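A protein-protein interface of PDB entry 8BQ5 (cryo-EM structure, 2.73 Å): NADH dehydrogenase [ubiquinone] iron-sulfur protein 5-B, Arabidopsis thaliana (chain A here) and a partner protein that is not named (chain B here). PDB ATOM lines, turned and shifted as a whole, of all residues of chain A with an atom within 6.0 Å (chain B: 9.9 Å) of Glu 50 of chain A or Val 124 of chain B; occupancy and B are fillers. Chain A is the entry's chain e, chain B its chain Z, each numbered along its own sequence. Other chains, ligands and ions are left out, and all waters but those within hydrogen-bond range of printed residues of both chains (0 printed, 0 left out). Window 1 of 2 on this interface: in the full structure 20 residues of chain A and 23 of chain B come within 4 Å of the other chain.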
ATOM      1  N   ASP A  40     -20.983  -3.208   4.337  1.00  0.00           N
ATOM      2  CA  ASP A  40     -19.573  -2.887   4.545  1.00  0.00           C
ATOM      3  C   ASP A  40     -19.232  -1.506   3.991  1.00  0.00           C
ATOM      4  O   ASP A  40     -18.528  -0.718   4.637  1.00  0.00           O
ATOM      5  CB  ASP A  40     -18.695  -3.959   3.905  1.00  0.00           C
ATOM      6  CG  ASP A  40     -18.296  -5.039   4.884  1.00  0.00           C
ATOM      7  OD1 ASP A  40     -17.395  -5.838   4.558  1.00  0.00           O
ATOM      8  OD2 ASP A  40     -18.887  -5.090   5.982  1.00  0.00           O
ATOM      9  N   GLU A  43     -20.807   1.052   6.240  1.00  0.00           N
ATOM     10  CA  GLU A  43     -20.062   1.110   7.491  1.00  0.00           C
ATOM     11  C   GLU A  43     -18.768   1.891   7.324  1.00  0.00           C
ATOM     12  O   GLU A  43     -18.362   2.633   8.225  1.00  0.00           O
ATOM     13  CB  GLU A  43     -19.780  -0.307   7.994  1.00  0.00           C
ATOM     14  CG  GLU A  43     -19.038  -0.377   9.318  1.00  0.00           C
ATOM     15  CD  GLU A  43     -19.751   0.347  10.442  1.00  0.00           C
ATOM     16  OE1 GLU A  43     -20.996   0.435  10.413  1.00  0.00           O
ATOM     17  OE2 GLU A  43     -19.060   0.827  11.362  1.00  0.00           O
ATOM     18  N   HIS A  47     -19.238   4.631   9.814  1.00  0.00           N
ATOM     19  CA  HIS A  47     -18.696   4.017  11.031  1.00  0.00           C
ATOM     20  C   HIS A  47     -19.770   3.776  12.088  1.00  0.00           C
ATOM     21  O   HIS A  47     -19.497   3.849  13.287  1.00  0.00           O
ATOM     22  CB  HIS A  47     -17.566   4.855  11.635  1.00  0.00           C
ATOM     23  CG  HIS A  47     -16.528   5.282  10.647  1.00  0.00           C
ATOM     24  ND1 HIS A  47     -15.697   4.389  10.011  1.00  0.00           N
ATOM     25  CD2 HIS A  47     -16.173   6.510  10.203  1.00  0.00           C
ATOM     26  CE1 HIS A  47     -14.880   5.046   9.209  1.00  0.00           C
ATOM     27  NE2 HIS A  47     -15.147   6.336   9.307  1.00  0.00           N
ATOM     28  N   SER A  48     -20.996   3.478  11.660  1.00  0.00           N
ATOM     29  CA  SER A  48     -22.114   3.464  12.596  1.00  0.00           C
ATOM     30  C   SER A  48     -22.000   2.313  13.592  1.00  0.00           C
ATOM     31  O   SER A  48     -22.182   2.505  14.800  1.00  0.00           O
ATOM     32  CB  SER A  48     -23.433   3.391  11.829  1.00  0.00           C
ATOM     33  OG  SER A  48     -24.528   3.330  12.722  1.00  0.00           O
ATOM     34  N   LYS A  49     -21.686   1.110  13.107  1.00  0.00           N
ATOM     35  CA  LYS A  49     -21.651  -0.047  13.996  1.00  0.00           C
ATOM     36  C   LYS A  49     -20.426  -0.025  14.901  1.00  0.00           C
ATOM     37  O   LYS A  49     -20.508  -0.413  16.073  1.00  0.00           O
ATOM     38  CB  LYS A  49     -21.710  -1.337  13.181  1.00  0.00           C
ATOM     39  CG  LYS A  49     -23.063  -1.565  12.529  1.00  0.00           C
ATOM     40  CD  LYS A  49     -23.091  -2.831  11.693  1.00  0.00           C
ATOM     41  CE  LYS A  49     -21.835  -2.986  10.864  1.00  0.00           C
ATOM     42  NZ  LYS A  49     -22.015  -2.404   9.508  1.00  0.00           N
ATOM     43  N   GLU A  50     -19.285   0.426  14.381  1.00  0.00           N
ATOM     44  CA  GLU A  50     -18.099   0.578  15.218  1.00  0.00           C
ATOM     45  C   GLU A  50     -18.367   1.530  16.378  1.00  0.00           C
ATOM     46  O   GLU A  50     -18.085   1.212  17.543  1.00  0.00           O
ATOM     47  CB  GLU A  50     -16.932   1.076  14.365  1.00  0.00           C
ATOM     48  CG  GLU A  50     -15.664   1.362  15.142  1.00  0.00           C
ATOM     49  CD  GLU A  50     -14.537   1.845  14.253  1.00  0.00           C
ATOM     50  OE1 GLU A  50     -13.452   2.158  14.785  1.00  0.00           O
ATOM     51  OE2 GLU A  50     -14.731   1.906  13.021  1.00  0.00           O
ATOM     52  N   PHE A  51     -18.938   2.696  16.078  1.00  0.00           N
ATOM     53  CA  PHE A  51     -19.221   3.672  17.123  1.00  0.00           C
ATOM     54  C   PHE A  51     -20.287   3.159  18.082  1.00  0.00           C
ATOM     55  O   PHE A  51     -20.217   3.418  19.285  1.00  0.00           O
ATOM     56  CB  PHE A  51     -19.646   5.004  16.507  1.00  0.00           C
ATOM     57  CG  PHE A  51     -18.528   5.743  15.830  1.00  0.00           C
ATOM     58  CD1 PHE A  51     -17.213   5.345  15.993  1.00  0.00           C
ATOM     59  CD2 PHE A  51     -18.795   6.839  15.030  1.00  0.00           C
ATOM     60  CE1 PHE A  51     -16.190   6.025  15.369  1.00  0.00           C
ATOM     61  CE2 PHE A  51     -17.776   7.523  14.405  1.00  0.00           C
ATOM     62  CZ  PHE A  51     -16.472   7.116  14.574  1.00  0.00           C
ATOM     63  N   GLN A  52     -21.282   2.428  17.570  1.00  0.00           N
ATOM     64  CA  GLN A  52     -22.307   1.869  18.447  1.00  0.00           C
ATOM     65  C   GLN A  52     -21.715   0.863  19.428  1.00  0.00           C
ATOM     66  O   GLN A  52     -22.055   0.867  20.618  1.00  0.00           O
ATOM     67  CB  GLN A  52     -23.407   1.212  17.617  1.00  0.00           C
ATOM     68  CG  GLN A  52     -24.601   0.771  18.439  1.00  0.00           C
ATOM     69  CD  GLN A  52     -25.900   0.867  17.674  1.00  0.00           C
ATOM     70  OE1 GLN A  52     -25.941   1.399  16.568  1.00  0.00           O
ATOM     71  NE2 GLN A  52     -26.973   0.353  18.261  1.00  0.00           N
ATOM     72  N   ARG A  53     -20.829  -0.011  18.948  1.00  0.00           N
ATOM     73  CA  ARG A  53     -20.210  -0.994  19.830  1.00  0.00           C
ATOM     74  C   ARG A  53     -19.313  -0.321  20.864  1.00  0.00           C
ATOM     75  O   ARG A  53     -19.320  -0.692  22.049  1.00  0.00           O
ATOM     76  CB  ARG A  53     -19.431  -2.010  18.995  1.00  0.00           C
ATOM     77  CG  ARG A  53     -18.283  -2.687  19.710  1.00  0.00           C
ATOM     78  CD  ARG A  53     -17.506  -3.564  18.744  1.00  0.00           C
ATOM     79  NE  ARG A  53     -16.526  -4.404  19.420  1.00  0.00           N
ATOM     80  CZ  ARG A  53     -16.736  -5.665  19.772  1.00  0.00           C
ATOM     81  NH1 ARG A  53     -17.896  -6.261  19.549  1.00  0.00           N
ATOM     82  NH2 ARG A  53     -15.757  -6.347  20.359  1.00  0.00           N
ATOM     83  N   ARG A  54     -18.541   0.685  20.442  1.00  0.00           N
ATOM     84  CA  ARG A  54     -17.714   1.404  21.406  1.00  0.00           C
ATOM     85  C   ARG A  54     -18.562   2.154  22.426  1.00  0.00           C
ATOM     86  O   ARG A  54     -18.180   2.258  23.597  1.00  0.00           O
ATOM     87  CB  ARG A  54     -16.762   2.352  20.680  1.00  0.00           C
ATOM     88  CG  ARG A  54     -15.551   1.646  20.094  1.00  0.00           C
ATOM     89  CD  ARG A  54     -14.969   2.383  18.900  1.00  0.00           C
ATOM     90  NE  ARG A  54     -13.953   3.354  19.287  1.00  0.00           N
ATOM     91  CZ  ARG A  54     -13.133   3.956  18.438  1.00  0.00           C
ATOM     92  NH1 ARG A  54     -13.148   3.676  17.146  1.00  0.00           N
ATOM     93  NH2 ARG A  54     -12.272   4.861  18.897  1.00  0.00           N
ATOM     94  N   ASN A  55     -19.721   2.669  22.011  1.00  0.00           N
ATOM     95  CA  ASN A  55     -20.625   3.297  22.963  1.00  0.00           C
ATOM     96  C   ASN A  55     -21.212   2.278  23.929  1.00  0.00           C
ATOM     97  O   ASN A  55     -21.455   2.605  25.093  1.00  0.00           O
ATOM     98  CB  ASN A  55     -21.735   4.041  22.224  1.00  0.00           C
ATOM     99  CG  ASN A  55     -21.231   5.288  21.525  1.00  0.00           C
ATOM    100  OD1 ASN A  55     -20.123   5.752  21.788  1.00  0.00           O
ATOM    101  ND2 ASN A  55     -22.041   5.835  20.630  1.00  0.00           N
ATOM    102  N   PHE B  97       1.436   0.380  17.246  1.00  0.00           N
ATOM    103  CA  PHE B  97      -0.009   0.222  17.168  1.00  0.00           C
ATOM    104  C   PHE B  97      -0.440  -1.168  17.612  1.00  0.00           C
ATOM    105  O   PHE B  97      -1.497  -1.319  18.228  1.00  0.00           O
ATOM    106  CB  PHE B  97      -0.512   0.506  15.756  1.00  0.00           C
ATOM    107  CG  PHE B  97      -1.992   0.334  15.611  1.00  0.00           C
ATOM    108  CD1 PHE B  97      -2.854   1.358  15.958  1.00  0.00           C
ATOM    109  CD2 PHE B  97      -2.524  -0.856  15.149  1.00  0.00           C
ATOM    110  CE1 PHE B  97      -4.217   1.203  15.840  1.00  0.00           C
ATOM    111  CE2 PHE B  97      -3.885  -1.017  15.028  1.00  0.00           C
ATOM    112  CZ  PHE B  97      -4.733   0.015  15.372  1.00  0.00           C
ATOM    113  N   TRP B 101      -2.972  -1.839  20.584  1.00  0.00           N
ATOM    114  CA  TRP B 101      -4.190  -2.585  20.314  1.00  0.00           C
ATOM    115  C   TRP B 101      -4.341  -3.756  21.272  1.00  0.00           C
ATOM    116  O   TRP B 101      -5.454  -4.069  21.701  1.00  0.00           O
ATOM    117  CB  TRP B 101      -4.199  -3.066  18.866  1.00  0.00           C
ATOM    118  CG  TRP B 101      -5.486  -3.701  18.477  1.00  0.00           C
ATOM    119  CD1 TRP B 101      -5.670  -4.985  18.063  1.00  0.00           C
ATOM    120  CD2 TRP B 101      -6.780  -3.090  18.483  1.00  0.00           C
ATOM    121  NE1 TRP B 101      -6.999  -5.211  17.801  1.00  0.00           N
ATOM    122  CE2 TRP B 101      -7.701  -4.062  18.051  1.00  0.00           C
ATOM    123  CE3 TRP B 101      -7.248  -1.812  18.804  1.00  0.00           C
ATOM    124  CZ2 TRP B 101      -9.062  -3.799  17.935  1.00  0.00           C
ATOM    125  CZ3 TRP B 101      -8.600  -1.552  18.687  1.00  0.00           C
ATOM    126  CH2 TRP B 101      -9.491  -2.542  18.257  1.00  0.00           C
ATOM    127  N   TYR B 104      -5.642  -2.215  24.480  1.00  0.00           N
ATOM    128  CA  TYR B 104      -7.065  -1.888  24.420  1.00  0.00           C
ATOM    129  C   TYR B 104      -7.922  -3.149  24.389  1.00  0.00           C
ATOM    130  O   TYR B 104      -9.028  -3.165  24.941  1.00  0.00           O
ATOM    131  CB  TYR B 104      -7.370  -1.003  23.209  1.00  0.00           C
ATOM    132  CG  TYR B 104      -8.855  -0.826  22.966  1.00  0.00           C
ATOM    133  CD1 TYR B 104      -9.579   0.132  23.663  1.00  0.00           C
ATOM    134  CD2 TYR B 104      -9.531  -1.612  22.043  1.00  0.00           C
ATOM    135  CE1 TYR B 104     -10.934   0.298  23.452  1.00  0.00           C
ATOM    136  CE2 TYR B 104     -10.884  -1.454  21.826  1.00  0.00           C
ATOM    137  CZ  TYR B 104     -11.581  -0.498  22.532  1.00  0.00           C
ATOM    138  OH  TYR B 104     -12.929  -0.335  22.318  1.00  0.00           O
ATOM    139  N   GLU B 108     -10.848  -3.960  27.036  1.00  0.00           N
ATOM    140  CA  GLU B 108     -12.205  -4.323  26.643  1.00  0.00           C
ATOM    141  C   GLU B 108     -12.606  -5.671  27.226  1.00  0.00           C
ATOM    142  O   GLU B 108     -13.752  -5.854  27.650  1.00  0.00           O
ATOM    143  CB  GLU B 108     -12.325  -4.342  25.120  1.00  0.00           C
ATOM    144  CG  GLU B 108     -13.754  -4.438  24.622  1.00  0.00           C
ATOM    145  CD  GLU B 108     -13.882  -5.243  23.345  1.00  0.00           C
ATOM    146  OE1 GLU B 108     -14.857  -6.012  23.226  1.00  0.00           O
ATOM    147  OE2 GLU B 108     -13.012  -5.103  22.461  1.00  0.00           O
ATOM    148  N   TRP B 118     -20.913 -11.073  24.233  1.00  0.00           N
ATOM    149  CA  TRP B 118     -19.910 -10.157  23.714  1.00  0.00           C
ATOM    150  C   TRP B 118     -18.770 -10.914  23.037  1.00  0.00           C
ATOM    151  O   TRP B 118     -18.543 -12.104  23.270  1.00  0.00           O
ATOM    152  CB  TRP B 118     -19.354  -9.272  24.828  1.00  0.00           C
ATOM    153  CG  TRP B 118     -18.719  -8.015  24.321  1.00  0.00           C
ATOM    154  CD1 TRP B 118     -17.387  -7.720  24.308  1.00  0.00           C
ATOM    155  CD2 TRP B 118     -19.386  -6.883  23.750  1.00  0.00           C
ATOM    156  NE1 TRP B 118     -17.183  -6.476  23.765  1.00  0.00           N
ATOM    157  CE2 TRP B 118     -18.394  -5.940  23.415  1.00  0.00           C
ATOM    158  CE3 TRP B 118     -20.724  -6.575  23.489  1.00  0.00           C
ATOM    159  CZ2 TRP B 118     -18.698  -4.711  22.835  1.00  0.00           C
ATOM    160  CZ3 TRP B 118     -21.023  -5.354  22.911  1.00  0.00           C
ATOM    161  CH2 TRP B 118     -20.015  -4.438  22.592  1.00  0.00           C
ATOM    162  N   LYS B 119     -18.050 -10.192  22.180  1.00  0.00           N
ATOM    163  CA  LYS B 119     -16.902 -10.719  21.452  1.00  0.00           C
ATOM    164  C   LYS B 119     -15.816  -9.656  21.467  1.00  0.00           C
ATOM    165  O   LYS B 119     -16.022  -8.556  20.944  1.00  0.00           O
ATOM    166  CB  LYS B 119     -17.283 -11.086  20.014  1.00  0.00           C
ATOM    167  CG  LYS B 119     -18.016 -12.410  19.878  1.00  0.00           C
ATOM    168  CD  LYS B 119     -18.938 -12.405  18.667  1.00  0.00           C
ATOM    169  CE  LYS B 119     -19.520 -13.783  18.408  1.00  0.00           C
ATOM    170  NZ  LYS B 119     -18.489 -14.712  17.867  1.00  0.00           N
ATOM    171  N   VAL B 120     -14.667  -9.977  22.058  1.00  0.00           N
ATOM    172  CA  VAL B 120     -13.612  -8.986  22.221  1.00  0.00           C
ATOM    173  C   VAL B 120     -12.929  -8.741  20.882  1.00  0.00           C
ATOM    174  O   VAL B 120     -12.379  -9.663  20.267  1.00  0.00           O
ATOM    175  CB  VAL B 120     -12.610  -9.440  23.293  1.00  0.00           C
ATOM    176  CG1 VAL B 120     -11.420  -8.498  23.343  1.00  0.00           C
ATOM    177  CG2 VAL B 120     -13.292  -9.512  24.651  1.00  0.00           C
ATOM    178  N   GLY B 121     -12.954  -7.490  20.430  1.00  0.00           N
ATOM    179  CA  GLY B 121     -12.368  -7.140  19.146  1.00  0.00           C
ATOM    180  C   GLY B 121     -13.077  -7.731  17.946  1.00  0.00           C
ATOM    181  O   GLY B 121     -12.419  -8.221  17.020  1.00  0.00           O
ATOM    182  N   GLU B 122     -14.407  -7.703  17.943  1.00  0.00           N
ATOM    183  CA  GLU B 122     -15.161  -8.169  16.786  1.00  0.00           C
ATOM    184  C   GLU B 122     -15.022  -7.176  15.637  1.00  0.00           C
ATOM    185  O   GLU B 122     -15.186  -5.966  15.824  1.00  0.00           O
ATOM    186  CB  GLU B 122     -16.634  -8.361  17.151  1.00  0.00           C
ATOM    187  CG  GLU B 122     -17.553  -8.588  15.955  1.00  0.00           C
ATOM    188  CD  GLU B 122     -18.798  -9.391  16.300  1.00  0.00           C
ATOM    189  OE1 GLU B 122     -19.658  -8.884  17.051  1.00  0.00           O
ATOM    190  OE2 GLU B 122     -18.914 -10.537  15.819  1.00  0.00           O
ATOM    191  N   ASN B 123     -14.706  -7.686  14.449  1.00  0.00           N
ATOM    192  CA  ASN B 123     -14.643  -6.851  13.257  1.00  0.00           C
ATOM    193  C   ASN B 123     -16.058  -6.533  12.793  1.00  0.00           C
ATOM    194  O   ASN B 123     -16.862  -7.443  12.564  1.00  0.00           O
ATOM    195  CB  ASN B 123     -13.856  -7.550  12.150  1.00  0.00           C
ATOM    196  CG  ASN B 123     -13.284  -6.575  11.136  1.00  0.00           C
ATOM    197  OD1 ASN B 123     -13.924  -5.586  10.779  1.00  0.00           O
ATOM    198  ND2 ASN B 123     -12.073  -6.850  10.668  1.00  0.00           N
ATOM    199  N   VAL B 124     -16.369  -5.243  12.659  1.00  0.00           N
ATOM    200  CA  VAL B 124     -17.692  -4.857  12.187  1.00  0.00           C
ATOM    201  C   VAL B 124     -17.828  -5.027  10.680  1.00  0.00           C
ATOM    202  O   VAL B 124     -18.942  -4.930  10.152  1.00  0.00           O
ATOM    203  CB  VAL B 124     -18.023  -3.410  12.588  1.00  0.00           C
ATOM    204  CG1 VAL B 124     -18.085  -3.279  14.104  1.00  0.00           C
ATOM    205  CG2 VAL B 124     -17.008  -2.448  12.000  1.00  0.00           C
ATOM    206  N   TYR B 125     -16.730  -5.289   9.977  1.00  0.00           N
ATOM    207  CA  TYR B 125     -16.764  -5.439   8.529  1.00  0.00           C
ATOM    208  C   TYR B 125     -16.908  -6.908   8.155  1.00  0.00           C
ATOM    209  O   TYR B 125     -16.138  -7.756   8.616  1.00  0.00           O
ATOM    210  CB  TYR B 125     -15.503  -4.843   7.906  1.00  0.00           C
ATOM    211  CG  TYR B 125     -15.460  -3.335   7.993  1.00  0.00           C
ATOM    212  CD1 TYR B 125     -16.295  -2.554   7.207  1.00  0.00           C
ATOM    213  CD2 TYR B 125     -14.594  -2.692   8.870  1.00  0.00           C
ATOM    214  CE1 TYR B 125     -16.267  -1.178   7.284  1.00  0.00           C
ATOM    215  CE2 TYR B 125     -14.561  -1.313   8.954  1.00  0.00           C
ATOM    216  CZ  TYR B 125     -15.400  -0.563   8.159  1.00  0.00           C
ATOM    217  OH  TYR B 125     -15.372   0.810   8.237  1.00  0.00           O
ATOM    218  N   ASN B 126     -17.904  -7.203   7.316  1.00  0.00           N
ATOM    219  CA  ASN B 126     -18.195  -8.588   6.958  1.00  0.00           C
ATOM    220  C   ASN B 126     -17.067  -9.207   6.146  1.00  0.00           C
ATOM    221  O   ASN B 126     -16.736 -10.382   6.327  1.00  0.00           O
ATOM    222  CB  ASN B 126     -19.512  -8.658   6.191  1.00  0.00           C
ATOM    223  CG  ASN B 126     -20.668  -8.099   6.981  1.00  0.00           C
ATOM    224  OD1 ASN B 126     -21.236  -7.069   6.626  1.00  0.00           O
ATOM    225  ND2 ASN B 126     -21.022  -8.774   8.068  1.00  0.00           N
ATOM    226  N   SER B 127     -16.464  -8.430   5.243  1.00  0.00           N
ATOM    227  CA  SER B 127     -15.359  -8.945   4.444  1.00  0.00           C
ATOM    228  C   SER B 127     -14.139  -9.276   5.293  1.00  0.00           C
ATOM    229  O   SER B 127     -13.239  -9.978   4.818  1.00  0.00           O
ATOM    230  CB  SER B 127     -14.982  -7.937   3.359  1.00  0.00           C
ATOM    231  OG  SER B 127     -14.045  -6.994   3.845  1.00  0.00           O
ATOM    232  N   GLY B 128     -14.083  -8.784   6.530  1.00  0.00           N
ATOM    233  CA  GLY B 128     -13.006  -9.112   7.439  1.00  0.00           C
ATOM    234  C   GLY B 128     -11.716  -8.363   7.208  1.00  0.00           C
ATOM    235  O   GLY B 128     -10.755  -8.574   7.955  1.00  0.00           O
ATOM    236  N   ARG B 129     -11.664  -7.492   6.207  1.00  0.00           N
ATOM    237  CA  ARG B 129     -10.449  -6.752   5.908  1.00  0.00           C
ATOM    238  C   ARG B 129     -10.166  -5.723   6.998  1.00  0.00           C
ATOM    239  O   ARG B 129     -11.077  -5.107   7.555  1.00  0.00           O
ATOM    240  CB  ARG B 129     -10.579  -6.095   4.536  1.00  0.00           C
ATOM    241  CG  ARG B 129      -9.388  -5.303   4.060  1.00  0.00           C
ATOM    242  CD  ARG B 129      -9.665  -4.791   2.664  1.00  0.00           C
ATOM    243  NE  ARG B 129      -8.536  -4.033   2.135  1.00  0.00           N
ATOM    244  CZ  ARG B 129      -8.426  -3.632   0.876  1.00  0.00           C
ATOM    245  NH1 ARG B 129      -9.359  -3.910  -0.019  1.00  0.00           N
ATOM    246  NH2 ARG B 129      -7.356  -2.937   0.507  1.00  0.00           N
ATOM    247  N   TRP B 130      -8.884  -5.558   7.315  1.00  0.00           N
ATOM    248  CA  TRP B 130      -8.483  -4.721   8.436  1.00  0.00           C
ATOM    249  C   TRP B 130      -8.565  -3.246   8.067  1.00  0.00           C
ATOM    250  O   TRP B 130      -8.105  -2.834   6.998  1.00  0.00           O
ATOM    251  CB  TRP B 130      -7.065  -5.066   8.887  1.00  0.00           C
ATOM    252  CG  TRP B 130      -6.623  -4.263  10.071  1.00  0.00           C
ATOM    253  CD1 TRP B 130      -6.847  -4.553  11.385  1.00  0.00           C
ATOM    254  CD2 TRP B 130      -5.900  -3.027  10.052  1.00  0.00           C
ATOM    255  NE1 TRP B 130      -6.302  -3.579  12.185  1.00  0.00           N
ATOM    256  CE2 TRP B 130      -5.715  -2.630  11.390  1.00  0.00           C
ATOM    257  CE3 TRP B 130      -5.388  -2.218   9.032  1.00  0.00           C
ATOM    258  CZ2 TRP B 130      -5.040  -1.462  11.736  1.00  0.00           C
ATOM    259  CZ3 TRP B 130      -4.717  -1.060   9.377  1.00  0.00           C
ATOM    260  CH2 TRP B 130      -4.551  -0.691  10.719  1.00  0.00           C
ATOM    261  N   MET B 131      -9.154  -2.456   8.956  1.00  0.00           N
ATOM    262  CA  MET B 131      -9.142  -1.007   8.863  1.00  0.00           C
ATOM    263  C   MET B 131      -8.732  -0.414  10.201  1.00  0.00           C
ATOM    264  O   MET B 131      -9.007  -0.993  11.256  1.00  0.00           O
ATOM    265  CB  MET B 131     -10.514  -0.449   8.459  1.00  0.00           C
ATOM    266  CG  MET B 131     -11.031  -0.969   7.133  1.00  0.00           C
ATOM    267  SD  MET B 131     -10.876   0.273   5.839  1.00  0.00           S
ATOM    268  CE  MET B 131     -10.365  -0.739   4.456  1.00  0.00           C
ATOM    269  N   PRO B 132      -8.065   0.738  10.183  1.00  0.00           N
ATOM    270  CA  PRO B 132      -7.746   1.409  11.436  1.00  0.00           C
ATOM    271  C   PRO B 132      -9.013   1.764  12.184  1.00  0.00           C
ATOM    272  O   PRO B 132     -10.081   1.955  11.575  1.00  0.00           O
ATOM    273  CB  PRO B 132      -6.992   2.668  10.984  1.00  0.00           C
ATOM    274  CG  PRO B 132      -6.524   2.399   9.613  1.00  0.00           C
ATOM    275  CD  PRO B 132      -7.321   1.277   9.033  1.00  0.00           C
ATOM    276  N   PRO B 133      -8.952   1.835  13.512  1.00  0.00           N
ATOM    277  CA  PRO B 133     -10.120   2.293  14.273  1.00  0.00           C
ATOM    278  C   PRO B 133     -10.487   3.722  13.900  1.00  0.00           C
ATOM    279  O   PRO B 133      -9.619   4.577  13.717  1.00  0.00           O
ATOM    280  CB  PRO B 133      -9.666   2.180  15.735  1.00  0.00           C
ATOM    281  CG  PRO B 133      -8.346   1.460  15.707  1.00  0.00           C
ATOM    282  CD  PRO B 133      -7.760   1.688  14.361  1.00  0.00           C
ATOM    283  N   ALA B 134     -11.788   3.974  13.790  1.00  0.00           N
ATOM    284  CA  ALA B 134     -12.269   5.304  13.452  1.00  0.00           C
ATOM    285  C   ALA B 134     -12.185   6.225  14.665  1.00  0.00           C
ATOM    286  O   ALA B 134     -12.423   5.814  15.802  1.00  0.00           O
ATOM    287  CB  ALA B 134     -13.703   5.238  12.932  1.00  0.00           C
ATOM    288  N   THR B 135     -11.811   7.488  14.425  1.00  0.00           N
ATOM    289  CA  THR B 135     -11.536   8.407  15.565  1.00  0.00           C
ATOM    290  C   THR B 135     -12.736   9.266  15.968  1.00  0.00           C
ATOM    291  O   THR B 135     -12.736   9.730  17.120  1.00  0.00           O
ATOM    292  CB  THR B 135     -10.333   9.313  15.261  1.00  0.00           C
ATOM    293  OG1 THR B 135     -10.725  10.321  14.327  1.00  0.00           O
ATOM    294  CG2 THR B 135      -9.149   8.553  14.705  1.00  0.00           C
ATOM    295  N   GLY B 136     -13.692   9.509  15.078  1.00  0.00           N
ATOM    296  CA  GLY B 136     -14.770  10.406  15.438  1.00  0.00           C
ATOM    297  C   GLY B 136     -14.448  11.871  15.263  1.00  0.00           C
ATOM    298  O   GLY B 136     -15.262  12.723  15.635  1.00  0.00           O
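CA of Tyr 125 of chain B touches OD2 of Asp 40 of chain A (3.3 Å). Glu 43 of chain A touches Val 124 of chain B. O of Glu 43 of chain A touches OH of Tyr 125 of chain B, at 3.5 Å. Val 124 of chain B touches Lys 49 of chain A. Val 124 of chain B touches Glu 50 of chain A (CG1 to N, 3.9 Å). Glu 50 of chain A touches Pro 133 of chain B (OE1 to CA, 3.4 Å). Ala 134 of chain B touches Phe 51 of chain A (CB to CE1, 3.6 Å). Phe 51 of chain A touches Gly 136 of chain B. NE1 of Trp 118 of chain B touches NH2 of Arg 53 of chain A, 3.7 Å away. Arg 53 of chain A touches Val 120 of chain B (NH2 to C, 3.7 Å).
OE1 of Glu 108 of chain B is in salt-bridge range of NH2 of Arg 53 of chain A (3.0 Å). O of Lys 119 of chain B lies close to NH1 of Arg 53 of chain A (3.3 Å). N of Asn 126 of chain B sits at hydrogen-bond distance from OD2 of Asp 40 of chain A (2.7 Å). The side-chain carboxylate (OD1) of Asp 40 of chain A lies within hydrogen-bond range of the backbone NH (N) of Ser 127 of chain B. The side-chain carboxylate (OE1) of Glu 50 of chain A is in hydrogen-bond range of the backbone NH (N) of Ala 134 of chain B, 2.7 Å away. The backbone carbonyl oxygen (O) of Ala 134 of chain B is in hydrogen-bond range of the guanidinium group (NH1) of Arg 54 of chain A, at 2.6 Å. The backbone NH (N) of Gly 121 of chain B sits close to the guanidinium group (NH2) of Arg 53 of chain A, 3.0 Å away. N of Glu 122 of chain B sits close to NH2 of Arg 53 of chain A, at 3.1 Å.
Of the printed residues of chain B, Glu 50 of chain A touches Val 124, Pro 133 and Ala 134. Printed residues of chain A within 4 Å of Val 124 of chain B: Glu 43 (3.9 Å), Lys 49 (3.6 Å) and Glu 50 (3.9 Å). Lys 49 of chain A touches just one residue of chain B: Val 124 (3.6 Å). Printed residues of chain A within 4 Å of Glu 108 of chain B: Arg 53 (3.0 Å). Of the printed residues of chain A, Ala 134 of chain B touches His 47, Glu 50, Phe 51 and Arg 54. Of the printed residues of chain A, Glu 122 of chain B touches Arg 53. Of the printed residues of chain A, Gly 136 of chain B touches Phe 51 (3.7 Å). Printed residues of chain B within 4 Å of Phe 51 of chain A: Ala 134 (3.6 Å) and Gly 136 (3.7 Å). The nearest residue of chain B that does not touch Glu 50 of chain A is Pro 132 of chain B (4.7 Å). The nearest residue of chain A that does not touch Val 124 of chain B is Asp 40 of chain A (4.2 Å). The nearest printed residue of chain A that does not touch Tyr 104 of chain B is Arg 53 of chain A (6.2 Å).
Of the 11 printed residues of chain A, 8 touch a printed residue of chain B. Hydrophobic or aromatic side chains of chain A that line the printed part of chain B: His 47 and Phe 51. Hydrophobic or aromatic side chains of chain B that line the printed part of chain A: Tyr 104, Trp 118, Val 124, Tyr 125, Pro 133 and Ala 134. Among the printed residues, 20 pairs touch across the chains. Among the printed residues, Asp or Glu carboxylates within 4 Å of a Lys or Arg side-chain nitrogen of the other chain: Arg 53 of chain A with Glu 108 of chain B.
The side-chain carboxylate (OE1) of Glu 108 of chain B sits at hydrogen-bond distance from the indole nitrogen (NE1) of Trp 118 of chain B (2.4 Å). The backbone NH (N) of Gly 121 of chain B sits at hydrogen-bond distance from the side-chain carboxylate (OE2) of Glu 108 of chain B. The side-chain amide oxygen (OD1) of Asn 123 of chain B is in hydrogen-bond range of the backbone NH (N) of Tyr 125 of chain B, 2.9 Å away. The side-chain carboxylate of Glu 43 of chain A is in salt-bridge range of the side-chain amino group of Lys 49 of chain A (3.1 Å). The backbone carbonyl oxygen of Phe 51 of chain A sits close to the side-chain amide nitrogen of Asn 55 of chain A (3.3 Å).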
